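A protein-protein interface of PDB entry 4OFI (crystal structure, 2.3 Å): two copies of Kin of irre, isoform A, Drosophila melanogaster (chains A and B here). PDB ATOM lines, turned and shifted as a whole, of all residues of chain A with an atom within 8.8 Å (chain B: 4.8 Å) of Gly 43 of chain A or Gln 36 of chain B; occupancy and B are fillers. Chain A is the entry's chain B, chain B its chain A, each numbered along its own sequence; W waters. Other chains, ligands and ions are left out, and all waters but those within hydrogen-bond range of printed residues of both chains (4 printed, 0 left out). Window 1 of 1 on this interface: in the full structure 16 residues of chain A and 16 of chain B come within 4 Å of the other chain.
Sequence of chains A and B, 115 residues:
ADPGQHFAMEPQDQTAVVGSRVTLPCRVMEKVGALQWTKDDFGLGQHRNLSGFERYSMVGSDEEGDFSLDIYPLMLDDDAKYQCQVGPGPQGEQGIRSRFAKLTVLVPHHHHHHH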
ATOM      1  N   ALA A  34      16.509 -10.079   6.633  1.00  0.00           N
ATOM      2  CA  ALA A  34      15.342 -10.566   7.361  1.00  0.00           C
ATOM      3  C   ALA A  34      15.537 -12.028   7.732  1.00  0.00           C
ATOM      4  O   ALA A  34      16.046 -12.813   6.936  1.00  0.00           O
ATOM      5  CB  ALA A  34      14.088 -10.400   6.529  1.00  0.00           C
ATOM      6  N   LEU A  35      15.136 -12.390   8.946  1.00  0.00           N
ATOM      7  CA  LEU A  35      15.350 -13.745   9.438  1.00  0.00           C
ATOM      8  C   LEU A  35      14.079 -14.598   9.380  1.00  0.00           C
ATOM      9  O   LEU A  35      12.970 -14.100   9.567  1.00  0.00           O
ATOM     10  CB  LEU A  35      15.925 -13.710  10.855  1.00  0.00           C
ATOM     11  CG  LEU A  35      16.287 -15.038  11.518  1.00  0.00           C
ATOM     12  CD1 LEU A  35      17.420 -14.857  12.518  1.00  0.00           C
ATOM     13  CD2 LEU A  35      15.068 -15.653  12.184  1.00  0.00           C
ATOM     14  N   GLN A  36      14.257 -15.889   9.126  1.00  0.00           N
ATOM     15  CA  GLN A  36      13.145 -16.820   9.032  1.00  0.00           C
ATOM     16  C   GLN A  36      13.621 -18.235   9.335  1.00  0.00           C
ATOM     17  O   GLN A  36      14.766 -18.578   9.042  1.00  0.00           O
ATOM     18  CB  GLN A  36      12.545 -16.748   7.625  1.00  0.00           C
ATOM     19  CG  GLN A  36      11.493 -17.777   7.315  1.00  0.00           C
ATOM     20  CD  GLN A  36      10.761 -17.466   6.029  1.00  0.00           C
ATOM     21  OE1 GLN A  36       9.571 -17.742   5.903  1.00  0.00           O
ATOM     22  NE2 GLN A  36      11.470 -16.887   5.063  1.00  0.00           N
ATOM     23  N   TRP A  37      12.750 -19.045   9.935  1.00  0.00           N
ATOM     24  CA  TRP A  37      13.004 -20.474  10.118  1.00  0.00           C
ATOM     25  C   TRP A  37      12.300 -21.261   9.020  1.00  0.00           C
ATOM     26  O   TRP A  37      11.203 -20.894   8.590  1.00  0.00           O
ATOM     27  CB  TRP A  37      12.465 -20.964  11.475  1.00  0.00           C
ATOM     28  CG  TRP A  37      13.351 -20.686  12.659  1.00  0.00           C
ATOM     29  CD1 TRP A  37      13.345 -19.565  13.442  1.00  0.00           C
ATOM     30  CD2 TRP A  37      14.361 -21.549  13.202  1.00  0.00           C
ATOM     31  NE1 TRP A  37      14.291 -19.675  14.433  1.00  0.00           N
ATOM     32  CE2 TRP A  37      14.929 -20.880  14.308  1.00  0.00           C
ATOM     33  CE3 TRP A  37      14.842 -22.817  12.857  1.00  0.00           C
ATOM     34  CZ2 TRP A  37      15.961 -21.438  15.074  1.00  0.00           C
ATOM     35  CZ3 TRP A  37      15.864 -23.373  13.625  1.00  0.00           C
ATOM     36  CH2 TRP A  37      16.411 -22.681  14.720  1.00  0.00           C
ATOM     37  N   THR A  38      12.920 -22.346   8.567  1.00  0.00           N
ATOM     38  CA  THR A  38      12.202 -23.322   7.750  1.00  0.00           C
ATOM     39  C   THR A  38      11.964 -24.611   8.522  1.00  0.00           C
ATOM     40  O   THR A  38      12.788 -25.024   9.339  1.00  0.00           O
ATOM     41  CB  THR A  38      12.929 -23.664   6.428  1.00  0.00           C
ATOM     42  OG1 THR A  38      14.255 -24.124   6.708  1.00  0.00           O
ATOM     43  CG2 THR A  38      12.986 -22.452   5.509  1.00  0.00           C
ATOM     44  N   LYS A  39      10.823 -25.234   8.261  1.00  0.00           N
ATOM     45  CA  LYS A  39      10.518 -26.551   8.796  1.00  0.00           C
ATOM     46  C   LYS A  39      10.238 -27.463   7.613  1.00  0.00           C
ATOM     47  O   LYS A  39       9.315 -27.213   6.839  1.00  0.00           O
ATOM     48  CB  LYS A  39       9.300 -26.486   9.714  1.00  0.00           C
ATOM     49  CG  LYS A  39       8.642 -27.834   9.939  1.00  0.00           C
ATOM     50  CD  LYS A  39       7.534 -27.752  10.980  1.00  0.00           C
ATOM     51  CE  LYS A  39       6.736 -29.043  11.017  1.00  0.00           C
ATOM     52  NZ  LYS A  39       5.379 -28.827  11.568  1.00  0.00           N
ATOM     53  N   ASP A  40      11.038 -28.513   7.467  1.00  0.00           N
ATOM     54  CA  ASP A  40      11.023 -29.297   6.242  1.00  0.00           C
ATOM     55  C   ASP A  40      11.026 -28.362   5.019  1.00  0.00           C
ATOM     56  O   ASP A  40      10.297 -28.577   4.051  1.00  0.00           O
ATOM     57  CB  ASP A  40       9.821 -30.249   6.211  1.00  0.00           C
ATOM     58  CG  ASP A  40       9.925 -31.365   7.250  1.00  0.00           C
ATOM     59  OD1 ASP A  40      11.060 -31.706   7.656  1.00  0.00           O
ATOM     60  OD2 ASP A  40       8.871 -31.905   7.663  1.00  0.00           O
ATOM     61  N   ASP A  41      11.846 -27.316   5.084  1.00  0.00           N
ATOM     62  CA  ASP A  41      12.016 -26.388   3.967  1.00  0.00           C
ATOM     63  C   ASP A  41      10.788 -25.514   3.695  1.00  0.00           C
ATOM     64  O   ASP A  41      10.688 -24.888   2.639  1.00  0.00           O
ATOM     65  CB  ASP A  41      12.403 -27.148   2.699  1.00  0.00           C
ATOM     66  CG  ASP A  41      13.659 -27.965   2.873  1.00  0.00           C
ATOM     67  OD1 ASP A  41      14.656 -27.408   3.368  1.00  0.00           O
ATOM     68  OD2 ASP A  41      13.647 -29.166   2.528  1.00  0.00           O
ATOM     69  N   PHE A  42       9.855 -25.479   4.641  1.00  0.00           N
ATOM     70  CA  PHE A  42       8.707 -24.591   4.539  1.00  0.00           C
ATOM     71  C   PHE A  42       8.946 -23.374   5.426  1.00  0.00           C
ATOM     72  O   PHE A  42       9.215 -23.516   6.618  1.00  0.00           O
ATOM     73  CB  PHE A  42       7.428 -25.310   4.963  1.00  0.00           C
ATOM     74  CG  PHE A  42       6.164 -24.563   4.624  1.00  0.00           C
ATOM     75  CD1 PHE A  42       5.739 -23.499   5.402  1.00  0.00           C
ATOM     76  CD2 PHE A  42       5.401 -24.928   3.527  1.00  0.00           C
ATOM     77  CE1 PHE A  42       4.575 -22.818   5.094  1.00  0.00           C
ATOM     78  CE2 PHE A  42       4.237 -24.249   3.214  1.00  0.00           C
ATOM     79  CZ  PHE A  42       3.823 -23.195   4.002  1.00  0.00           C
ATOM     80  N   GLY A  43       8.855 -22.185   4.833  1.00  0.00           N
ATOM     81  CA  GLY A  43       9.092 -20.942   5.545  1.00  0.00           C
ATOM     82  C   GLY A  43       8.026 -20.614   6.573  1.00  0.00           C
ATOM     83  O   GLY A  43       6.847 -20.493   6.247  1.00  0.00           O
ATOM     84  N   LEU A  44       8.447 -20.456   7.824  1.00  0.00           N
ATOM     85  CA  LEU A  44       7.510 -20.231   8.920  1.00  0.00           C
ATOM     86  C   LEU A  44       7.062 -18.774   9.042  1.00  0.00           C
ATOM     87  O   LEU A  44       6.004 -18.488   9.607  1.00  0.00           O
ATOM     88  CB  LEU A  44       8.111 -20.711  10.246  1.00  0.00           C
ATOM     89  CG  LEU A  44       8.345 -22.220  10.372  1.00  0.00           C
ATOM     90  CD1 LEU A  44       8.688 -22.583  11.818  1.00  0.00           C
ATOM     91  CD2 LEU A  44       7.117 -22.991   9.898  1.00  0.00           C
ATOM     92  N   GLY A  45       7.870 -17.854   8.527  1.00  0.00           N
ATOM     93  CA  GLY A  45       7.522 -16.444   8.579  1.00  0.00           C
ATOM     94  C   GLY A  45       8.692 -15.553   8.943  1.00  0.00           C
ATOM     95  O   GLY A  45       9.551 -15.938   9.727  1.00  0.00           O
ATOM     96  N   GLN A  46       8.729 -14.358   8.364  1.00  0.00           N
ATOM     97  CA  GLN A  46       9.799 -13.408   8.645  1.00  0.00           C
ATOM     98  C   GLN A  46       9.411 -12.470   9.776  1.00  0.00           C
ATOM     99  O   GLN A  46       8.245 -12.396  10.155  1.00  0.00           O
ATOM    100  CB  GLN A  46      10.145 -12.592   7.394  1.00  0.00           C
ATOM    101  CG  GLN A  46      10.888 -13.379   6.331  1.00  0.00           C
ATOM    102  CD  GLN A  46      11.139 -12.574   5.078  1.00  0.00           C
ATOM    103  OE1 GLN A  46      10.327 -11.728   4.694  1.00  0.00           O
ATOM    104  NE2 GLN A  46      12.270 -12.830   4.430  1.00  0.00           N
ATOM    105  N   ASN A  49       6.912 -12.901  12.683  1.00  0.00           N
ATOM    106  CA  ASN A  49       5.494 -13.076  12.388  1.00  0.00           C
ATOM    107  C   ASN A  49       5.203 -14.494  11.916  1.00  0.00           C
ATOM    108  O   ASN A  49       5.452 -14.834  10.757  1.00  0.00           O
ATOM    109  CB  ASN A  49       5.016 -12.058  11.347  1.00  0.00           C
ATOM    110  CG  ASN A  49       3.502 -11.960  11.279  1.00  0.00           C
ATOM    111  OD1 ASN A  49       2.790 -12.904  11.629  1.00  0.00           O
ATOM    112  ND2 ASN A  49       3.004 -10.811  10.827  1.00  0.00           N
ATOM    113  N   LEU A  50       4.681 -15.316  12.824  1.00  0.00           N
ATOM    114  CA  LEU A  50       4.411 -16.720  12.533  1.00  0.00           C
ATOM    115  C   LEU A  50       2.910 -17.010  12.488  1.00  0.00           C
ATOM    116  O   LEU A  50       2.435 -17.991  13.066  1.00  0.00           O
ATOM    117  CB  LEU A  50       5.104 -17.621  13.560  1.00  0.00           C
ATOM    118  CG  LEU A  50       6.603 -17.373  13.748  1.00  0.00           C
ATOM    119  CD1 LEU A  50       7.263 -18.555  14.430  1.00  0.00           C
ATOM    120  CD2 LEU A  50       7.284 -17.101  12.416  1.00  0.00           C
ATOM    121  N   SER A  51       2.177 -16.147  11.791  1.00  0.00           N
ATOM    122  CA  SER A  51       0.727 -16.270  11.652  1.00  0.00           C
ATOM    123  C   SER A  51       0.332 -17.666  11.194  1.00  0.00           C
ATOM    124  O   SER A  51       0.888 -18.196  10.230  1.00  0.00           O
ATOM    125  CB  SER A  51       0.206 -15.228  10.654  1.00  0.00           C
ATOM    126  OG  SER A  51      -1.193 -15.346  10.436  1.00  0.00           O
ATOM    127  N   PHE A  53       0.755 -20.429  12.772  1.00  0.00           N
ATOM    128  CA  PHE A  53       1.460 -21.399  13.600  1.00  0.00           C
ATOM    129  C   PHE A  53       1.303 -21.015  15.065  1.00  0.00           C
ATOM    130  O   PHE A  53       2.182 -20.378  15.650  1.00  0.00           O
ATOM    131  CB  PHE A  53       2.940 -21.479  13.216  1.00  0.00           C
ATOM    132  CG  PHE A  53       3.166 -21.833  11.781  1.00  0.00           C
ATOM    133  CD1 PHE A  53       2.988 -23.136  11.340  1.00  0.00           C
ATOM    134  CD2 PHE A  53       3.543 -20.867  10.865  1.00  0.00           C
ATOM    135  CE1 PHE A  53       3.187 -23.468  10.011  1.00  0.00           C
ATOM    136  CE2 PHE A  53       3.745 -21.191   9.533  1.00  0.00           C
ATOM    137  CZ  PHE A  53       3.566 -22.496   9.105  1.00  0.00           C
ATOM    138  N   TYR A  56       4.146 -21.973  17.601  1.00  0.00           N
ATOM    139  CA  TYR A  56       5.504 -21.483  17.400  1.00  0.00           C
ATOM    140  C   TYR A  56       5.587 -19.999  17.732  1.00  0.00           C
ATOM    141  O   TYR A  56       4.643 -19.243  17.491  1.00  0.00           O
ATOM    142  CB  TYR A  56       5.965 -21.678  15.954  1.00  0.00           C
ATOM    143  CG  TYR A  56       5.839 -23.082  15.423  1.00  0.00           C
ATOM    144  CD1 TYR A  56       5.590 -24.158  16.273  1.00  0.00           C
ATOM    145  CD2 TYR A  56       5.968 -23.333  14.063  1.00  0.00           C
ATOM    146  CE1 TYR A  56       5.473 -25.448  15.778  1.00  0.00           C
ATOM    147  CE2 TYR A  56       5.855 -24.612  13.553  1.00  0.00           C
ATOM    148  CZ  TYR A  56       5.604 -25.666  14.408  1.00  0.00           C
ATOM    149  OH  TYR A  56       5.500 -26.930  13.881  1.00  0.00           O
ATOM    150  N   GLN A  83      15.839 -25.175   9.883  1.00  0.00           N
ATOM    151  CA  GLN A  83      16.999 -24.350   9.564  1.00  0.00           C
ATOM    152  C   GLN A  83      16.724 -22.869   9.819  1.00  0.00           C
ATOM    153  O   GLN A  83      15.626 -22.377   9.559  1.00  0.00           O
ATOM    154  CB  GLN A  83      17.424 -24.575   8.115  1.00  0.00           C
ATOM    155  CG  GLN A  83      18.645 -23.791   7.685  1.00  0.00           C
ATOM    156  CD  GLN A  83      19.021 -24.053   6.234  1.00  0.00           C
ATOM    157  OE1 GLN A  83      18.284 -23.695   5.313  1.00  0.00           O
ATOM    158  NE2 GLN A  83      20.170 -24.684   6.027  1.00  0.00           N
ATOM    159  N   GLN A  85      17.413 -19.103   8.781  1.00  0.00           N
ATOM    160  CA  GLN A  85      17.836 -18.404   7.572  1.00  0.00           C
ATOM    161  C   GLN A  85      17.807 -16.888   7.723  1.00  0.00           C
ATOM    162  O   GLN A  85      16.884 -16.334   8.318  1.00  0.00           O
ATOM    163  CB  GLN A  85      16.961 -18.820   6.382  1.00  0.00           C
ATOM    164  CG  GLN A  85      16.997 -20.309   6.071  1.00  0.00           C
ATOM    165  CD  GLN A  85      16.113 -20.678   4.891  1.00  0.00           C
ATOM    166  OE1 GLN A  85      15.401 -19.834   4.342  1.00  0.00           O
ATOM    167  NE2 GLN A  85      16.153 -21.947   4.497  1.00  0.00           N
ATOM    168  N   ALA B  34      -0.141 -16.418   4.108  1.00  0.00           N
ATOM    169  CA  ALA B  34       0.898 -15.624   3.466  1.00  0.00           C
ATOM    170  C   ALA B  34       1.669 -16.469   2.459  1.00  0.00           C
ATOM    171  O   ALA B  34       2.121 -17.575   2.765  1.00  0.00           O
ATOM    172  CB  ALA B  34       1.845 -15.038   4.510  1.00  0.00           C
ATOM    173  N   LEU B  35       1.819 -15.939   1.251  1.00  0.00           N
ATOM    174  CA  LEU B  35       2.494 -16.660   0.186  1.00  0.00           C
ATOM    175  C   LEU B  35       3.977 -16.307   0.155  1.00  0.00           C
ATOM    176  O   LEU B  35       4.365 -15.168   0.435  1.00  0.00           O
ATOM    177  CB  LEU B  35       1.833 -16.358  -1.161  1.00  0.00           C
ATOM    178  CG  LEU B  35       2.300 -17.114  -2.405  1.00  0.00           C
ATOM    179  CD1 LEU B  35       1.164 -17.199  -3.411  1.00  0.00           C
ATOM    180  CD2 LEU B  35       3.544 -16.474  -3.028  1.00  0.00           C
ATOM    181  N   GLN B  36       4.799 -17.292  -0.187  1.00  0.00           N
ATOM    182  CA  GLN B  36       6.239 -17.095  -0.272  1.00  0.00           C
ATOM    183  C   GLN B  36       6.850 -18.111  -1.225  1.00  0.00           C
ATOM    184  O   GLN B  36       6.423 -19.266  -1.272  1.00  0.00           O
ATOM    185  CB  GLN B  36       6.875 -17.226   1.118  1.00  0.00           C
ATOM    186  CG  GLN B  36       8.387 -17.074   1.132  1.00  0.00           C
ATOM    187  CD  GLN B  36       8.965 -17.036   2.537  1.00  0.00           C
ATOM    188  OE1 GLN B  36       9.985 -16.394   2.776  1.00  0.00           O
ATOM    189  NE2 GLN B  36       8.314 -17.729   3.476  1.00  0.00           N
ATOM    190  N   TRP B  37       7.847 -17.677  -1.986  1.00  0.00           N
ATOM    191  CA  TRP B  37       8.607 -18.576  -2.843  1.00  0.00           C
ATOM    192  C   TRP B  37       9.865 -19.059  -2.127  1.00  0.00           C
ATOM    193  O   TRP B  37      10.430 -18.340  -1.299  1.00  0.00           O
ATOM    194  CB  TRP B  37       9.009 -17.866  -4.141  1.00  0.00           C
ATOM    195  CG  TRP B  37       7.921 -17.797  -5.188  1.00  0.00           C
ATOM    196  CD1 TRP B  37       6.923 -16.869  -5.277  1.00  0.00           C
ATOM    197  CD2 TRP B  37       7.735 -18.692  -6.295  1.00  0.00           C
ATOM    198  NE1 TRP B  37       6.123 -17.134  -6.368  1.00  0.00           N
ATOM    199  CE2 TRP B  37       6.605 -18.244  -7.013  1.00  0.00           C
ATOM    200  CE3 TRP B  37       8.414 -19.827  -6.749  1.00  0.00           C
ATOM    201  CZ2 TRP B  37       6.134 -18.893  -8.155  1.00  0.00           C
ATOM    202  CZ3 TRP B  37       7.950 -20.468  -7.894  1.00  0.00           C
ATOM    203  CH2 TRP B  37       6.820 -19.999  -8.581  1.00  0.00           C
ATOM    204  N   THR B  38      10.309 -20.273  -2.442  1.00  0.00           N
ATOM    205  CA  THR B  38      11.638 -20.698  -2.020  1.00  0.00           C
ATOM    206  C   THR B  38      12.527 -20.961  -3.224  1.00  0.00           C
ATOM    207  O   THR B  38      12.069 -21.426  -4.267  1.00  0.00           O
ATOM    208  CB  THR B  38      11.617 -21.948  -1.115  1.00  0.00           C
ATOM    209  OG1 THR B  38      11.178 -23.088  -1.865  1.00  0.00           O
ATOM    210  CG2 THR B  38      10.707 -21.724   0.089  1.00  0.00           C
ATOM    211  N   GLY B  43      13.762 -19.202   1.700  1.00  0.00           N
ATOM    212  CA  GLY B  43      12.615 -18.320   1.575  1.00  0.00           C
ATOM    213  C   GLY B  43      13.015 -16.959   1.029  1.00  0.00           C
ATOM    214  O   GLY B  43      13.881 -16.286   1.598  1.00  0.00           O
ATOM    215  N   LEU B  44      12.378 -16.553  -0.066  1.00  0.00           N
ATOM    216  CA  LEU B  44      12.714 -15.303  -0.741  1.00  0.00           C
ATOM    217  C   LEU B  44      12.058 -14.082  -0.101  1.00  0.00           C
ATOM    218  O   LEU B  44      12.493 -12.953  -0.320  1.00  0.00           O
ATOM    219  CB  LEU B  44      12.334 -15.379  -2.226  1.00  0.00           C
ATOM    220  CG  LEU B  44      13.093 -16.418  -3.053  1.00  0.00           C
ATOM    221  CD1 LEU B  44      12.703 -16.339  -4.529  1.00  0.00           C
ATOM    222  CD2 LEU B  44      14.589 -16.227  -2.871  1.00  0.00           C
ATOM    223  N   GLY B  45      11.011 -14.304   0.685  1.00  0.00           N
ATOM    224  CA  GLY B  45      10.326 -13.207   1.344  1.00  0.00           C
ATOM    225  C   GLY B  45       8.832 -13.214   1.091  1.00  0.00           C
ATOM    226  O   GLY B  45       8.355 -13.827   0.139  1.00  0.00           O
ATOM    227  N   GLN B  46       8.088 -12.519   1.938  1.00  0.00           N
ATOM    228  CA  GLN B  46       6.634 -12.580   1.879  1.00  0.00           C
ATOM    229  C   GLN B  46       6.005 -11.302   1.352  1.00  0.00           C
ATOM    230  O   GLN B  46       4.794 -11.128   1.432  1.00  0.00           O
ATOM    231  CB  GLN B  46       6.062 -12.921   3.256  1.00  0.00           C
ATOM    232  CG  GLN B  46       6.399 -14.329   3.714  1.00  0.00           C
ATOM    233  CD  GLN B  46       6.066 -14.559   5.170  1.00  0.00           C
ATOM    234  OE1 GLN B  46       6.440 -13.771   6.032  1.00  0.00           O
ATOM    235  NE2 GLN B  46       5.353 -15.641   5.451  1.00  0.00           N
ATOM    236  N   GLN B  83       9.934 -23.224  -5.316  1.00  0.00           N
ATOM    237  CA  GLN B  83       8.630 -23.674  -4.862  1.00  0.00           C
ATOM    238  C   GLN B  83       7.777 -22.507  -4.399  1.00  0.00           C
ATOM    239  O   GLN B  83       8.275 -21.563  -3.785  1.00  0.00           O
ATOM    240  CB  GLN B  83       8.758 -24.710  -3.740  1.00  0.00           C
ATOM    241  CG  GLN B  83       7.460 -25.432  -3.433  1.00  0.00           C
ATOM    242  CD  GLN B  83       7.596 -26.414  -2.284  1.00  0.00           C
ATOM    243  OE1 GLN B  83       7.971 -26.037  -1.177  1.00  0.00           O
ATOM    244  NE2 GLN B  83       7.293 -27.681  -2.542  1.00  0.00           N
ATOM    245  N   CYS B  84       6.490 -22.578  -4.706  1.00  0.00           N
ATOM    246  CA  CYS B  84       5.547 -21.579  -4.240  1.00  0.00           C
ATOM    247  C   CYS B  84       4.827 -22.132  -3.014  1.00  0.00           C
ATOM    248  O   CYS B  84       4.289 -23.234  -3.053  1.00  0.00           O
ATOM    249  CB  CYS B  84       4.561 -21.222  -5.354  1.00  0.00           C
ATOM    250  SG  CYS B  84       3.359 -19.953  -4.920  1.00  0.00           S
ATOM    251  N   GLN B  85       4.839 -21.381  -1.919  1.00  0.00           N
ATOM    252  CA  GLN B  85       4.227 -21.847  -0.676  1.00  0.00           C
ATOM    253  C   GLN B  85       3.200 -20.845  -0.164  1.00  0.00           C
ATOM    254  O   GLN B  85       3.354 -19.642  -0.349  1.00  0.00           O
ATOM    255  CB  GLN B  85       5.297 -22.064   0.398  1.00  0.00           C
ATOM    256  CG  GLN B  85       6.484 -22.894  -0.052  1.00  0.00           C
ATOM    257  CD  GLN B  85       7.545 -23.025   1.030  1.00  0.00           C
ATOM    258  OE1 GLN B  85       7.503 -22.324   2.041  1.00  0.00           O
ATOM    259  NE2 GLN B  85       8.504 -23.930   0.823  1.00  0.00           N
HETATM  260  O   HOH W   1       6.489 -20.153   3.432  1.00  0.00           O
HETATM  261  O   HOH W   2      14.964 -13.737   2.617  1.00  0.00           O
HETATM  262  O   HOH W   3      14.270 -17.009   4.266  1.00  0.00           O
HETATM  263  O   HOH W   4      11.182 -25.162  -0.118  1.00  0.00           O
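The side-chain amide oxygen of Gln 36 of chain B is in hydrogen-bond range of the backbone NH of Gly 45 of chain B (3.1 Å).
The backbone carbonyl oxygen (O) of Gln 36 of chain B is in hydrogen-bond range of the backbone NH (N) of Gln 85 of chain B (2.7 Å).
The side-chain amide nitrogen (NE2) of Gln 85 of chain B lies within hydrogen-bond range of the side-chain amide oxygen (OE1) of Gln 83 of chain B (3.0 Å).
OE1 of Gln 36 of chain A lies within hydrogen-bond range of N of Gly 45 of chain A (3.1 Å).
The backbone NH (N) of Gln 85 of chain A sits at hydrogen-bond distance from the backbone carbonyl oxygen (O) of Gln 36 of chain A (2.7 Å).
The side-chain amide nitrogen of Gln 85 of chain A lies within hydrogen-bond range of the side-chain amide oxygen of Gln 83 of chain A (2.9 Å).
The side-chain amide oxygen (OE1) of Gln 36 of chain A sits at hydrogen-bond distance from the side-chain amide nitrogen (NE2) of Gln 36 of chain B (2.7 Å).
The side-chain amide oxygen (OE1) of Gln 85 of chain A lies within hydrogen-bond range of the backbone NH (N) of Gly 43 of chain B, at 3.2 Å.
The side-chain amide oxygen of Gln 46 of chain B lies within hydrogen-bond range of the backbone NH of Gln 46 of chain A (3.3 Å).
The side-chain amide nitrogen (NE2) of Gln 85 of chain B lies within hydrogen-bond range of the backbone carbonyl oxygen (O) of Asp 41 of chain A.
OE1 of Gln 85 of chain B lies within hydrogen-bond range of N of Gly 43 of chain A (3.1 Å).
Water W4 lies within hydrogen-bond range of OG1 of Thr 38 of chain B (2.7 Å), O of Asp 41 of chain A (2.8 Å), NE2 of Gln 85 of chain B (3.1 Å) and OE1 of Gln 83 of chain B (3.5 Å).
Water W1 lies within hydrogen-bond range of OE1 of Gln 85 of chain B (2.8 Å), O of Gly 43 of chain A (2.9 Å) and NE2 of Gln 36 of chain B (3.0 Å).
Water W3 lies within hydrogen-bond range of O of Gly 43 of chain B (2.8 Å), NE2 of Gln 36 of chain A (2.9 Å) and OE1 of Gln 85 of chain A (3.0 Å).
Water W2 bridges the backbone carbonyl oxygen of Gly 43 of chain B (3.0 Å) and the side-chain amide nitrogen of Gln 46 of chain A (3.4 Å).
Of the 12 printed residues of chain B, 5 touch a printed residue of chain A.
Printed residues of chain A that touch a printed residue of chain B: Gln 36, Asp 41, Phe 42, Gly 43, Gly 45, Gln 46 and Gln 85.
Printed residues of chain B within 4 Å of Gly 43 of chain A: Gln 36 and Gln 85.
Of chain A, only Gln 36 (2.7 Å) and Gly 43 (3.9 Å) come within 4 Å of Gln 36 of chain B.
Gly 45 of chain B touches just one residue of chain A: Gln 46 (3.7 Å).
Gln 85 of chain B touches just these residues of chain A: Asp 41 (3.0 Å), Phe 42 (3.6 Å) and Gly 43 (3.1 Å).
Of the printed residues of chain B, Phe 42 of chain A touches Gln 85 (3.6 Å).
Printed residues of chain A within 4 Å of Gly 43 of chain B: Gln 36 and Gln 85.
Printed residues of chain A within 4 Å of Gln 46 of chain B: Gly 45 (3.8 Å) and Gln 46 (3.3 Å).
Printed residues of chain B within 4 Å of Gln 36 of chain A: Gln 36 and Gly 43.
Of the printed residues of chain B, Gln 85 of chain A touches Gly 43.
Asp 40 of chain A touches none of the printed residues of chain B.
The nearest printed residue of chain B that does not touch Gly 43 of chain A is Thr 38 of chain B (5.1 Å).
The nearest residue of chain A that does not touch Gln 36 of chain B is Gln 46 of chain A (4.5 Å).
The nearest printed residue of chain A that does not touch Gln 46 of chain B is Gln 36 of chain A (4.7 Å).
Gln 36 of chain B touches its own counterpart, Gln 36 of chain A.
Gln 36 of chain A touches Gly 43 of chain B, and with the chains exchanged Gly 43 of chain A touches Gln 36 of chain B.
Gly 43 of chain A touches Gln 85 of chain B, and with the chains exchanged Gln 85 of chain A touches Gly 43 of chain B.
Gln 46 of chain B touches its own counterpart, Gln 46 of chain A.
Positions printed for both chains: 34, 35, 36, 37, 38, 43, 44, 45, 46, 83 and 85.
Of the 10 pairs that touch across the chains among the printed residues, 8 have their exchanged pair printed and touching as well.
Gln 36 of chain A touches Gly 43 of chain B (NE2 to CA, 3.9 Å).
Gln 85 of chain B touches Phe 42 of chain A (OE1 to CA, 3.6 Å).
Gly 43 of chain A touches Gln 36 of chain B (CA to NE2, 3.9 Å).
Gln 46 of chain B touches Gly 45 of chain A.
OE1 of Gln 46 of chain A touches CA of Gly 45 of chain B (3.7 Å).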
